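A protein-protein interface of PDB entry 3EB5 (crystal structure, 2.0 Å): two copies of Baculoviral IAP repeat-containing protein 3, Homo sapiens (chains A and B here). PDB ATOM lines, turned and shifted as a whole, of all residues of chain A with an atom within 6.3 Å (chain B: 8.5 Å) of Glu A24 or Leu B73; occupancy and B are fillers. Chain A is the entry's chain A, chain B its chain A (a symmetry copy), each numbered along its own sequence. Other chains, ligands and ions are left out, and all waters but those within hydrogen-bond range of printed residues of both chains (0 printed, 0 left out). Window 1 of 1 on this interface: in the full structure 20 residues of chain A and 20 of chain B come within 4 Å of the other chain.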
ATOM      1  N   ARG A  19      12.793  16.871 -27.670  1.00  0.00           N
ATOM      2  CA  ARG A  19      13.343  17.434 -28.899  1.00  0.00           C
ATOM      3  C   ARG A  19      14.660  18.166 -28.644  1.00  0.00           C
ATOM      4  O   ARG A  19      15.571  18.110 -29.469  1.00  0.00           O
ATOM      5  CB  ARG A  19      12.334  18.384 -29.538  1.00  0.00           C
ATOM      6  CG  ARG A  19      12.768  18.967 -30.869  1.00  0.00           C
ATOM      7  CD  ARG A  19      12.013  20.256 -31.155  1.00  0.00           C
ATOM      8  NE  ARG A  19      12.871  21.270 -31.769  1.00  0.00           N
ATOM      9  CZ  ARG A  19      13.716  22.053 -31.100  1.00  0.00           C
ATOM     10  NH1 ARG A  19      13.841  21.946 -29.780  1.00  0.00           N
ATOM     11  NH2 ARG A  19      14.447  22.947 -31.756  1.00  0.00           N
ATOM     12  N   ARG A  20      14.740  18.854 -27.504  1.00  0.00           N
ATOM     13  CA  ARG A  20      15.926  19.617 -27.117  1.00  0.00           C
ATOM     14  C   ARG A  20      17.109  18.709 -26.802  1.00  0.00           C
ATOM     15  O   ARG A  20      18.258  19.026 -27.141  1.00  0.00           O
ATOM     16  CB  ARG A  20      15.621  20.501 -25.912  1.00  0.00           C
ATOM     17  CG  ARG A  20      14.861  21.763 -26.249  1.00  0.00           C
ATOM     18  CD  ARG A  20      14.476  22.497 -24.981  1.00  0.00           C
ATOM     19  NE  ARG A  20      14.360  23.936 -25.195  1.00  0.00           N
ATOM     20  CZ  ARG A  20      13.217  24.578 -25.410  1.00  0.00           C
ATOM     21  NH1 ARG A  20      12.069  23.919 -25.443  1.00  0.00           N
ATOM     22  NH2 ARG A  20      13.222  25.891 -25.588  1.00  0.00           N
ATOM     23  N   LEU A  21      16.818  17.582 -26.155  1.00  0.00           N
ATOM     24  CA  LEU A  21      17.841  16.601 -25.816  1.00  0.00           C
ATOM     25  C   LEU A  21      18.311  15.808 -27.028  1.00  0.00           C
ATOM     26  O   LEU A  21      19.502  15.553 -27.156  1.00  0.00           O
ATOM     27  CB  LEU A  21      17.372  15.669 -24.694  1.00  0.00           C
ATOM     28  CG  LEU A  21      17.034  16.294 -23.333  1.00  0.00           C
ATOM     29  CD1 LEU A  21      16.856  15.202 -22.298  1.00  0.00           C
ATOM     30  CD2 LEU A  21      18.086  17.297 -22.861  1.00  0.00           C
ATOM     31  N   GLN A  22      17.391  15.436 -27.917  1.00  0.00           N
ATOM     32  CA  GLN A  22      17.753  14.790 -29.187  1.00  0.00           C
ATOM     33  C   GLN A  22      18.699  15.682 -29.990  1.00  0.00           C
ATOM     34  O   GLN A  22      19.715  15.221 -30.513  1.00  0.00           O
ATOM     35  CB  GLN A  22      16.509  14.472 -30.018  1.00  0.00           C
ATOM     36  CG  GLN A  22      15.755  13.227 -29.572  1.00  0.00           C
ATOM     37  CD  GLN A  22      14.361  13.128 -30.170  1.00  0.00           C
ATOM     38  OE1 GLN A  22      13.657  14.131 -30.325  1.00  0.00           O
ATOM     39  NE2 GLN A  22      13.951  11.911 -30.501  1.00  0.00           N
ATOM     40  N   GLU A  23      18.363  16.969 -30.043  1.00  0.00           N
ATOM     41  CA  GLU A  23      19.111  17.966 -30.796  1.00  0.00           C
ATOM     42  C   GLU A  23      20.544  18.148 -30.280  1.00  0.00           C
ATOM     43  O   GLU A  23      21.478  18.283 -31.073  1.00  0.00           O
ATOM     44  CB  GLU A  23      18.356  19.296 -30.757  1.00  0.00           C
ATOM     45  CG  GLU A  23      18.826  20.349 -31.748  1.00  0.00           C
ATOM     46  CD  GLU A  23      18.002  21.633 -31.673  1.00  0.00           C
ATOM     47  OE1 GLU A  23      16.759  21.550 -31.537  1.00  0.00           O
ATOM     48  OE2 GLU A  23      18.602  22.729 -31.756  1.00  0.00           O
ATOM     49  N   GLU A  24      20.715  18.150 -28.960  1.00  0.00           N
ATOM     50  CA  GLU A  24      22.038  18.357 -28.364  1.00  0.00           C
ATOM     51  C   GLU A  24      22.910  17.092 -28.403  1.00  0.00           C
ATOM     52  O   GLU A  24      24.110  17.144 -28.145  1.00  0.00           O
ATOM     53  CB  GLU A  24      21.919  18.910 -26.939  1.00  0.00           C
ATOM     54  CG  GLU A  24      21.693  17.860 -25.856  1.00  0.00           C
ATOM     55  CD  GLU A  24      21.977  18.385 -24.454  1.00  0.00           C
ATOM     56  OE1 GLU A  24      22.051  19.624 -24.282  1.00  0.00           O
ATOM     57  OE2 GLU A  24      22.125  17.558 -23.524  1.00  0.00           O
ATOM     58  N   ARG A  25      22.286  15.973 -28.751  1.00  0.00           N
ATOM     59  CA  ARG A  25      22.929  14.667 -28.819  1.00  0.00           C
ATOM     60  C   ARG A  25      23.198  14.261 -30.281  1.00  0.00           C
ATOM     61  O   ARG A  25      23.909  13.290 -30.547  1.00  0.00           O
ATOM     62  CB  ARG A  25      22.016  13.654 -28.120  1.00  0.00           C
ATOM     63  CG  ARG A  25      22.481  12.216 -28.083  1.00  0.00           C
ATOM     64  CD  ARG A  25      21.260  11.302 -28.137  1.00  0.00           C
ATOM     65  NE  ARG A  25      21.623   9.887 -28.133  1.00  0.00           N
ATOM     66  CZ  ARG A  25      20.788   8.894 -28.429  1.00  0.00           C
ATOM     67  NH1 ARG A  25      19.527   9.147 -28.767  1.00  0.00           N
ATOM     68  NH2 ARG A  25      21.220   7.639 -28.394  1.00  0.00           N
ATOM     69  N   THR A  26      22.638  15.024 -31.217  1.00  0.00           N
ATOM     70  CA  THR A  26      22.746  14.736 -32.647  1.00  0.00           C
ATOM     71  C   THR A  26      23.805  15.617 -33.301  1.00  0.00           C
ATOM     72  O   THR A  26      23.958  16.786 -32.943  1.00  0.00           O
ATOM     73  CB  THR A  26      21.376  14.925 -33.356  1.00  0.00           C
ATOM     74  OG1 THR A  26      20.395  14.096 -32.722  1.00  0.00           O
ATOM     75  CG2 THR A  26      21.448  14.548 -34.833  1.00  0.00           C
ATOM     76  N   LYS A  28      25.763  18.116 -35.448  1.00  0.00           N
ATOM     77  CA  LYS A  28      25.344  19.410 -35.967  1.00  0.00           C
ATOM     78  C   LYS A  28      25.640  19.607 -37.457  1.00  0.00           C
ATOM     79  O   LYS A  28      25.244  20.625 -38.025  1.00  0.00           O
ATOM     80  CB  LYS A  28      25.949  20.546 -35.133  1.00  0.00           C
ATOM     81  CG  LYS A  28      24.964  21.272 -34.204  1.00  0.00           C
ATOM     82  CD  LYS A  28      24.238  20.349 -33.222  1.00  0.00           C
ATOM     83  CE  LYS A  28      25.102  19.965 -32.019  1.00  0.00           C
ATOM     84  NZ  LYS A  28      24.442  18.924 -31.172  1.00  0.00           N
ATOM     85  N   VAL A  35      26.572  12.661 -31.643  1.00  0.00           N
ATOM     86  CA  VAL A  35      27.861  13.267 -31.336  1.00  0.00           C
ATOM     87  C   VAL A  35      28.749  12.222 -30.674  1.00  0.00           C
ATOM     88  O   VAL A  35      28.256  11.380 -29.914  1.00  0.00           O
ATOM     89  CB  VAL A  35      27.706  14.499 -30.407  1.00  0.00           C
ATOM     90  CG1 VAL A  35      26.901  15.577 -31.102  1.00  0.00           C
ATOM     91  CG2 VAL A  35      27.041  14.126 -29.085  1.00  0.00           C
ATOM     92  N   GLY A  43      36.464  22.135 -26.536  1.00  0.00           N
ATOM     93  CA  GLY A  43      35.696  21.181 -25.740  1.00  0.00           C
ATOM     94  C   GLY A  43      34.254  20.959 -26.177  1.00  0.00           C
ATOM     95  O   GLY A  43      33.475  20.333 -25.452  1.00  0.00           O
ATOM     96  N   HIS A  44      33.878  21.451 -27.354  1.00  0.00           N
ATOM     97  CA  HIS A  44      32.545  21.133 -27.861  1.00  0.00           C
ATOM     98  C   HIS A  44      32.388  19.689 -28.288  1.00  0.00           C
ATOM     99  O   HIS A  44      33.294  19.109 -28.857  1.00  0.00           O
ATOM    100  CB  HIS A  44      32.112  22.089 -28.958  1.00  0.00           C
ATOM    101  CG  HIS A  44      31.688  23.417 -28.429  1.00  0.00           C
ATOM    102  ND1 HIS A  44      32.207  24.606 -28.891  1.00  0.00           N
ATOM    103  CD2 HIS A  44      30.830  23.738 -27.435  1.00  0.00           C
ATOM    104  CE1 HIS A  44      31.661  25.606 -28.226  1.00  0.00           C
ATOM    105  NE2 HIS A  44      30.828  25.105 -27.333  1.00  0.00           N
ATOM    106  N   LEU A  45      31.235  19.118 -27.966  1.00  0.00           N
ATOM    107  CA  LEU A  45      30.851  17.792 -28.417  1.00  0.00           C
ATOM    108  C   LEU A  45      29.658  17.985 -29.341  1.00  0.00           C
ATOM    109  O   LEU A  45      28.511  17.981 -28.899  1.00  0.00           O
ATOM    110  CB  LEU A  45      30.514  16.909 -27.208  1.00  0.00           C
ATOM    111  CG  LEU A  45      29.947  15.485 -27.344  1.00  0.00           C
ATOM    112  CD1 LEU A  45      30.856  14.582 -28.157  1.00  0.00           C
ATOM    113  CD2 LEU A  45      29.705  14.899 -25.979  1.00  0.00           C
ATOM    114  N   VAL A  46      29.933  18.196 -30.626  1.00  0.00           N
ATOM    115  CA  VAL A  46      28.889  18.644 -31.553  1.00  0.00           C
ATOM    116  C   VAL A  46      28.831  17.880 -32.871  1.00  0.00           C
ATOM    117  O   VAL A  46      27.903  18.066 -33.658  1.00  0.00           O
ATOM    118  CB  VAL A  46      28.956  20.179 -31.811  1.00  0.00           C
ATOM    119  CG1 VAL A  46      28.604  20.940 -30.544  1.00  0.00           C
ATOM    120  CG2 VAL A  46      30.336  20.599 -32.341  1.00  0.00           C
ATOM    121  N   LEU A  73      28.538   8.266 -25.129  1.00  0.00           N
ATOM    122  CA  LEU A  73      27.436   8.537 -24.200  1.00  0.00           C
ATOM    123  C   LEU A  73      26.896   7.209 -23.669  1.00  0.00           C
ATOM    124  O   LEU A  73      26.692   6.254 -24.437  1.00  0.00           O
ATOM    125  CB  LEU A  73      26.311   9.308 -24.899  1.00  0.00           C
ATOM    126  CG  LEU A  73      26.542  10.778 -25.258  1.00  0.00           C
ATOM    127  CD1 LEU A  73      25.669  11.143 -26.447  1.00  0.00           C
ATOM    128  CD2 LEU A  73      26.254  11.697 -24.069  1.00  0.00           C
ATOM    129  N   LEU B  21      17.200   9.852 -22.347  1.00  0.00           N
ATOM    130  CA  LEU B  21      18.127  10.912 -22.722  1.00  0.00           C
ATOM    131  C   LEU B  21      18.576  11.742 -21.527  1.00  0.00           C
ATOM    132  O   LEU B  21      19.746  12.092 -21.442  1.00  0.00           O
ATOM    133  CB  LEU B  21      17.544  11.802 -23.825  1.00  0.00           C
ATOM    134  CG  LEU B  21      17.208  11.149 -25.174  1.00  0.00           C
ATOM    135  CD1 LEU B  21      16.906  12.222 -26.200  1.00  0.00           C
ATOM    136  CD2 LEU B  21      18.320  10.234 -25.685  1.00  0.00           C
ATOM    137  N   GLN B  22      17.662  12.040 -20.604  1.00  0.00           N
ATOM    138  CA  GLN B  22      18.017  12.715 -19.348  1.00  0.00           C
ATOM    139  C   GLN B  22      19.059  11.903 -18.581  1.00  0.00           C
ATOM    140  O   GLN B  22      20.053  12.446 -18.094  1.00  0.00           O
ATOM    141  CB  GLN B  22      16.781  12.933 -18.471  1.00  0.00           C
ATOM    142  CG  GLN B  22      15.913  14.112 -18.888  1.00  0.00           C
ATOM    143  CD  GLN B  22      14.539  14.099 -18.240  1.00  0.00           C
ATOM    144  OE1 GLN B  22      13.925  13.043 -18.060  1.00  0.00           O
ATOM    145  NE2 GLN B  22      14.045  15.280 -17.892  1.00  0.00           N
ATOM    146  N   GLU B  24      21.229   9.605 -19.687  1.00  0.00           N
ATOM    147  CA  GLU B  24      22.542   9.503 -20.331  1.00  0.00           C
ATOM    148  C   GLU B  24      23.310  10.835 -20.322  1.00  0.00           C
ATOM    149  O   GLU B  24      24.500  10.880 -20.623  1.00  0.00           O
ATOM    150  CB  GLU B  24      22.416   8.941 -21.751  1.00  0.00           C
ATOM    151  CG  GLU B  24      22.067   9.968 -22.824  1.00  0.00           C
ATOM    152  CD  GLU B  24      22.341   9.465 -24.236  1.00  0.00           C
ATOM    153  OE1 GLU B  24      22.509   8.236 -24.413  1.00  0.00           O
ATOM    154  OE2 GLU B  24      22.388  10.300 -25.169  1.00  0.00           O
ATOM    155  N   ARG B  25      22.611  11.901 -19.950  1.00  0.00           N
ATOM    156  CA  ARG B  25      23.149  13.255 -19.904  1.00  0.00           C
ATOM    157  C   ARG B  25      23.437  13.683 -18.452  1.00  0.00           C
ATOM    158  O   ARG B  25      24.077  14.708 -18.210  1.00  0.00           O
ATOM    159  CB  ARG B  25      22.132  14.189 -20.567  1.00  0.00           C
ATOM    160  CG  ARG B  25      22.478  15.661 -20.619  1.00  0.00           C
ATOM    161  CD  ARG B  25      21.190  16.473 -20.519  1.00  0.00           C
ATOM    162  NE  ARG B  25      21.437  17.912 -20.534  1.00  0.00           N
ATOM    163  CZ  ARG B  25      20.536  18.835 -20.206  1.00  0.00           C
ATOM    164  NH1 ARG B  25      19.312  18.482 -19.823  1.00  0.00           N
ATOM    165  NH2 ARG B  25      20.864  20.121 -20.255  1.00  0.00           N
ATOM    166  N   THR B  26      22.974  12.879 -17.496  1.00  0.00           N
ATOM    167  CA  THR B  26      23.110  13.177 -16.071  1.00  0.00           C
ATOM    168  C   THR B  26      24.261  12.385 -15.458  1.00  0.00           C
ATOM    169  O   THR B  26      24.494  11.231 -15.823  1.00  0.00           O
ATOM    170  CB  THR B  26      21.787  12.879 -15.313  1.00  0.00           C
ATOM    171  OG1 THR B  26      20.720  13.624 -15.910  1.00  0.00           O
ATOM    172  CG2 THR B  26      21.882  13.262 -13.839  1.00  0.00           C
ATOM    173  N   GLU B  34      24.867  17.733 -14.964  1.00  0.00           N
ATOM    174  CA  GLU B  34      25.072  17.023 -16.217  1.00  0.00           C
ATOM    175  C   GLU B  34      26.536  16.617 -16.438  1.00  0.00           C
ATOM    176  O   GLU B  34      27.464  17.233 -15.904  1.00  0.00           O
ATOM    177  CB  GLU B  34      24.496  17.789 -17.415  1.00  0.00           C
ATOM    178  CG  GLU B  34      25.117  19.142 -17.715  1.00  0.00           C
ATOM    179  CD  GLU B  34      24.509  19.794 -18.951  1.00  0.00           C
ATOM    180  OE1 GLU B  34      25.239  20.485 -19.699  1.00  0.00           O
ATOM    181  OE2 GLU B  34      23.296  19.614 -19.179  1.00  0.00           O
ATOM    182  N   VAL B  35      26.718  15.552 -17.210  1.00  0.00           N
ATOM    183  CA  VAL B  35      28.039  15.051 -17.565  1.00  0.00           C
ATOM    184  C   VAL B  35      28.816  16.163 -18.257  1.00  0.00           C
ATOM    185  O   VAL B  35      28.229  16.961 -18.998  1.00  0.00           O
ATOM    186  CB  VAL B  35      27.951  13.809 -18.490  1.00  0.00           C
ATOM    187  CG1 VAL B  35      27.261  12.671 -17.767  1.00  0.00           C
ATOM    188  CG2 VAL B  35      27.211  14.126 -19.786  1.00  0.00           C
ATOM    189  N   SER B  36      30.121  16.223 -18.005  1.00  0.00           N
ATOM    190  CA  SER B  36      30.974  17.234 -18.630  1.00  0.00           C
ATOM    191  C   SER B  36      32.452  16.846 -18.648  1.00  0.00           C
ATOM    192  O   SER B  36      33.305  17.657 -19.005  1.00  0.00           O
ATOM    193  CB  SER B  36      30.796  18.595 -17.947  1.00  0.00           C
ATOM    194  OG  SER B  36      31.265  18.528 -16.617  1.00  0.00           O
ATOM    195  N   ILE B  37      32.755  15.613 -18.256  1.00  0.00           N
ATOM    196  CA  ILE B  37      34.126  15.138 -18.239  1.00  0.00           C
ATOM    197  C   ILE B  37      34.224  13.864 -19.064  1.00  0.00           C
ATOM    198  O   ILE B  37      33.445  12.939 -18.865  1.00  0.00           O
ATOM    199  CB  ILE B  37      34.611  14.859 -16.789  1.00  0.00           C
ATOM    200  CG1 ILE B  37      34.763  16.162 -16.009  1.00  0.00           C
ATOM    201  CG2 ILE B  37      35.950  14.098 -16.778  1.00  0.00           C
ATOM    202  CD1 ILE B  37      35.788  17.153 -16.618  1.00  0.00           C
ATOM    203  N   LEU B  45      31.750   9.487 -21.064  1.00  0.00           N
ATOM    204  CA  LEU B  45      31.277  10.778 -20.598  1.00  0.00           C
ATOM    205  C   LEU B  45      30.138  10.491 -19.631  1.00  0.00           C
ATOM    206  O   LEU B  45      28.979  10.402 -20.031  1.00  0.00           O
ATOM    207  CB  LEU B  45      30.826  11.629 -21.792  1.00  0.00           C
ATOM    208  CG  LEU B  45      30.151  13.003 -21.633  1.00  0.00           C
ATOM    209  CD1 LEU B  45      31.014  13.977 -20.852  1.00  0.00           C
ATOM    210  CD2 LEU B  45      29.814  13.565 -22.988  1.00  0.00           C
ATOM    211  N   ARG B  70      37.443  18.257 -20.405  1.00  0.00           N
ATOM    212  CA  ARG B  70      36.209  18.925 -20.072  1.00  0.00           C
ATOM    213  C   ARG B  70      35.412  19.151 -21.353  1.00  0.00           C
ATOM    214  O   ARG B  70      35.897  19.796 -22.295  1.00  0.00           O
ATOM    215  CB  ARG B  70      36.537  20.263 -19.409  1.00  0.00           C
ATOM    216  CG  ARG B  70      35.344  21.078 -18.976  1.00  0.00           C
ATOM    217  CD  ARG B  70      34.667  20.503 -17.720  1.00  0.00           C
ATOM    218  NE  ARG B  70      34.192  21.578 -16.837  1.00  0.00           N
ATOM    219  CZ  ARG B  70      33.080  22.288 -17.031  1.00  0.00           C
ATOM    220  NH1 ARG B  70      32.302  22.056 -18.088  1.00  0.00           N
ATOM    221  NH2 ARG B  70      32.743  23.244 -16.166  1.00  0.00           N
ATOM    222  N   THR B  71      34.190  18.632 -21.390  1.00  0.00           N
ATOM    223  CA  THR B  71      33.339  18.866 -22.548  1.00  0.00           C
ATOM    224  C   THR B  71      32.033  19.613 -22.246  1.00  0.00           C
ATOM    225  O   THR B  71      31.538  19.594 -21.117  1.00  0.00           O
ATOM    226  CB  THR B  71      33.072  17.577 -23.352  1.00  0.00           C
ATOM    227  OG1 THR B  71      32.456  17.926 -24.607  1.00  0.00           O
ATOM    228  CG2 THR B  71      32.172  16.656 -22.601  1.00  0.00           C
ATOM    229  N   PHE B  72      31.504  20.276 -23.276  1.00  0.00           N
ATOM    230  CA  PHE B  72      30.249  21.022 -23.195  1.00  0.00           C
ATOM    231  C   PHE B  72      29.269  20.489 -24.245  1.00  0.00           C
ATOM    232  O   PHE B  72      29.597  20.417 -25.437  1.00  0.00           O
ATOM    233  CB  PHE B  72      30.489  22.534 -23.392  1.00  0.00           C
ATOM    234  CG  PHE B  72      31.736  23.048 -22.715  1.00  0.00           C
ATOM    235  CD1 PHE B  72      32.924  23.197 -23.429  1.00  0.00           C
ATOM    236  CD2 PHE B  72      31.734  23.363 -21.357  1.00  0.00           C
ATOM    237  CE1 PHE B  72      34.100  23.661 -22.802  1.00  0.00           C
ATOM    238  CE2 PHE B  72      32.908  23.825 -20.718  1.00  0.00           C
ATOM    239  CZ  PHE B  72      34.090  23.975 -21.446  1.00  0.00           C
ATOM    240  N   LEU B  73      28.085  20.081 -23.785  1.00  0.00           N
ATOM    241  CA  LEU B  73      26.976  19.721 -24.674  1.00  0.00           C
ATOM    242  C   LEU B  73      26.311  21.000 -25.183  1.00  0.00           C
ATOM    243  O   LEU B  73      26.059  21.937 -24.407  1.00  0.00           O
ATOM    244  CB  LEU B  73      25.943  18.863 -23.936  1.00  0.00           C
ATOM    245  CG  LEU B  73      26.304  17.417 -23.587  1.00  0.00           C
ATOM    246  CD1 LEU B  73      25.508  16.985 -22.368  1.00  0.00           C
ATOM    247  CD2 LEU B  73      26.048  16.475 -24.767  1.00  0.00           C
ATOM    248  N   SER B  74      26.032  21.040 -26.484  1.00  0.00           N
ATOM    249  CA  SER B  74      25.481  22.249 -27.100  1.00  0.00           C
ATOM    250  C   SER B  74      24.331  21.978 -28.066  1.00  0.00           C
ATOM    251  O   SER B  74      23.458  22.830 -28.236  1.00  0.00           O
ATOM    252  CB  SER B  74      26.590  23.053 -27.786  1.00  0.00           C
ATOM    253  OG  SER B  74      27.475  23.591 -26.812  1.00  0.00           O
ATOM    254  OXT SER B  74      24.243  20.917 -28.689  1.00  0.00           O
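The side-chain carboxylate (OE2) of Glu A24 lies within salt-bridge range of the guanidinium group (NE) of Arg B25, at 3.1 Å. The side-chain carboxylate (OE2) of Glu B24 is in salt-bridge range of the guanidinium group (NE) of Arg A25 (3.1 Å). The side-chain amino group (NZ) of Lys A28 lies within salt-bridge range of the chain-end carboxylate (OXT) of Ser B74 (3.2 Å). O of Gly A43 sits at hydrogen-bond distance from OG1 of Thr B71 (2.7 Å). The backbone carbonyl oxygen of Gly A43 is in hydrogen-bond range of the backbone NH of Phe B72 (2.9 Å). N of Leu A45 sits at hydrogen-bond distance from O of Phe B72.
The backbone carbonyl oxygen of Glu A23 lies within hydrogen-bond range of the side-chain amino group of Lys A28, 3.0 Å away. The backbone NH (N) of Val A35 sits at hydrogen-bond distance from the backbone carbonyl oxygen (O) of Arg A25 (2.9 Å). The side-chain hydroxyl (OG1) of Thr B26 is in hydrogen-bond range of the backbone carbonyl oxygen (O) of Gln B22, at 2.6 Å. The side-chain carboxylate (OE2) of Glu B34 lies within salt-bridge range of the guanidinium group (NH2) of Arg B25, at 2.7 Å. N of Val B35 sits at hydrogen-bond distance from O of Arg B25 (2.9 Å). The backbone carbonyl oxygen (O) of Ser B36 is in hydrogen-bond range of the backbone NH (N) of Thr B71, at 2.7 Å.
Among the printed residues, merely in contact across the chains: Leu A45 with Leu B45, Glu A24 with Ser B74, Leu A45 with Thr B71, His A44 with Ser B74, Leu A21 with Arg B25, Arg A25 with Leu B21, Leu A73 with Glu B24, Glu A24 with Leu B73, Gln A22 with Leu B21, Leu A21 with Gln B22, Gly A43 with Arg B70, Leu A21 with Leu B21 and His A44 with Phe B72.
Glu A24 touches just these residues of chain B: Arg B25, Leu B73 and Ser B74. Leu B73 touches just one residue of chain A: Glu A24 (3.6 Å). Of the printed residues of chain B, Arg A25 touches Leu B21 (3.5 Å) and Glu B24 (3.1 Å). Printed residues of chain A within 4 Å of Glu B24: Arg A25 (3.1 Å) and Leu A73 (3.6 Å). The nearest residue of chain A that does not touch Leu B73 is Leu A45 (4.2 Å).
Of the 15 printed residues of chain A, 9 touch a printed residue of chain B. Among the printed residues, Asp or Glu carboxylates within 4 Å of a Lys or Arg side-chain nitrogen of the other chain: Glu A24 with Arg B25 and Arg A25 with Glu B24.
Leu B21 touches its own counterpart, Leu A21. Glu A24 touches Arg B25, and with the chains exchanged Arg A25 touches Glu B24. Glu A24 touches Leu B73, and with the chains exchanged Leu A73 touches Glu B24. Leu A45 touches its own counterpart, Leu B45. Positions printed for both chains: 21, 22, 24, 25, 26, 35, 45 and 73.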
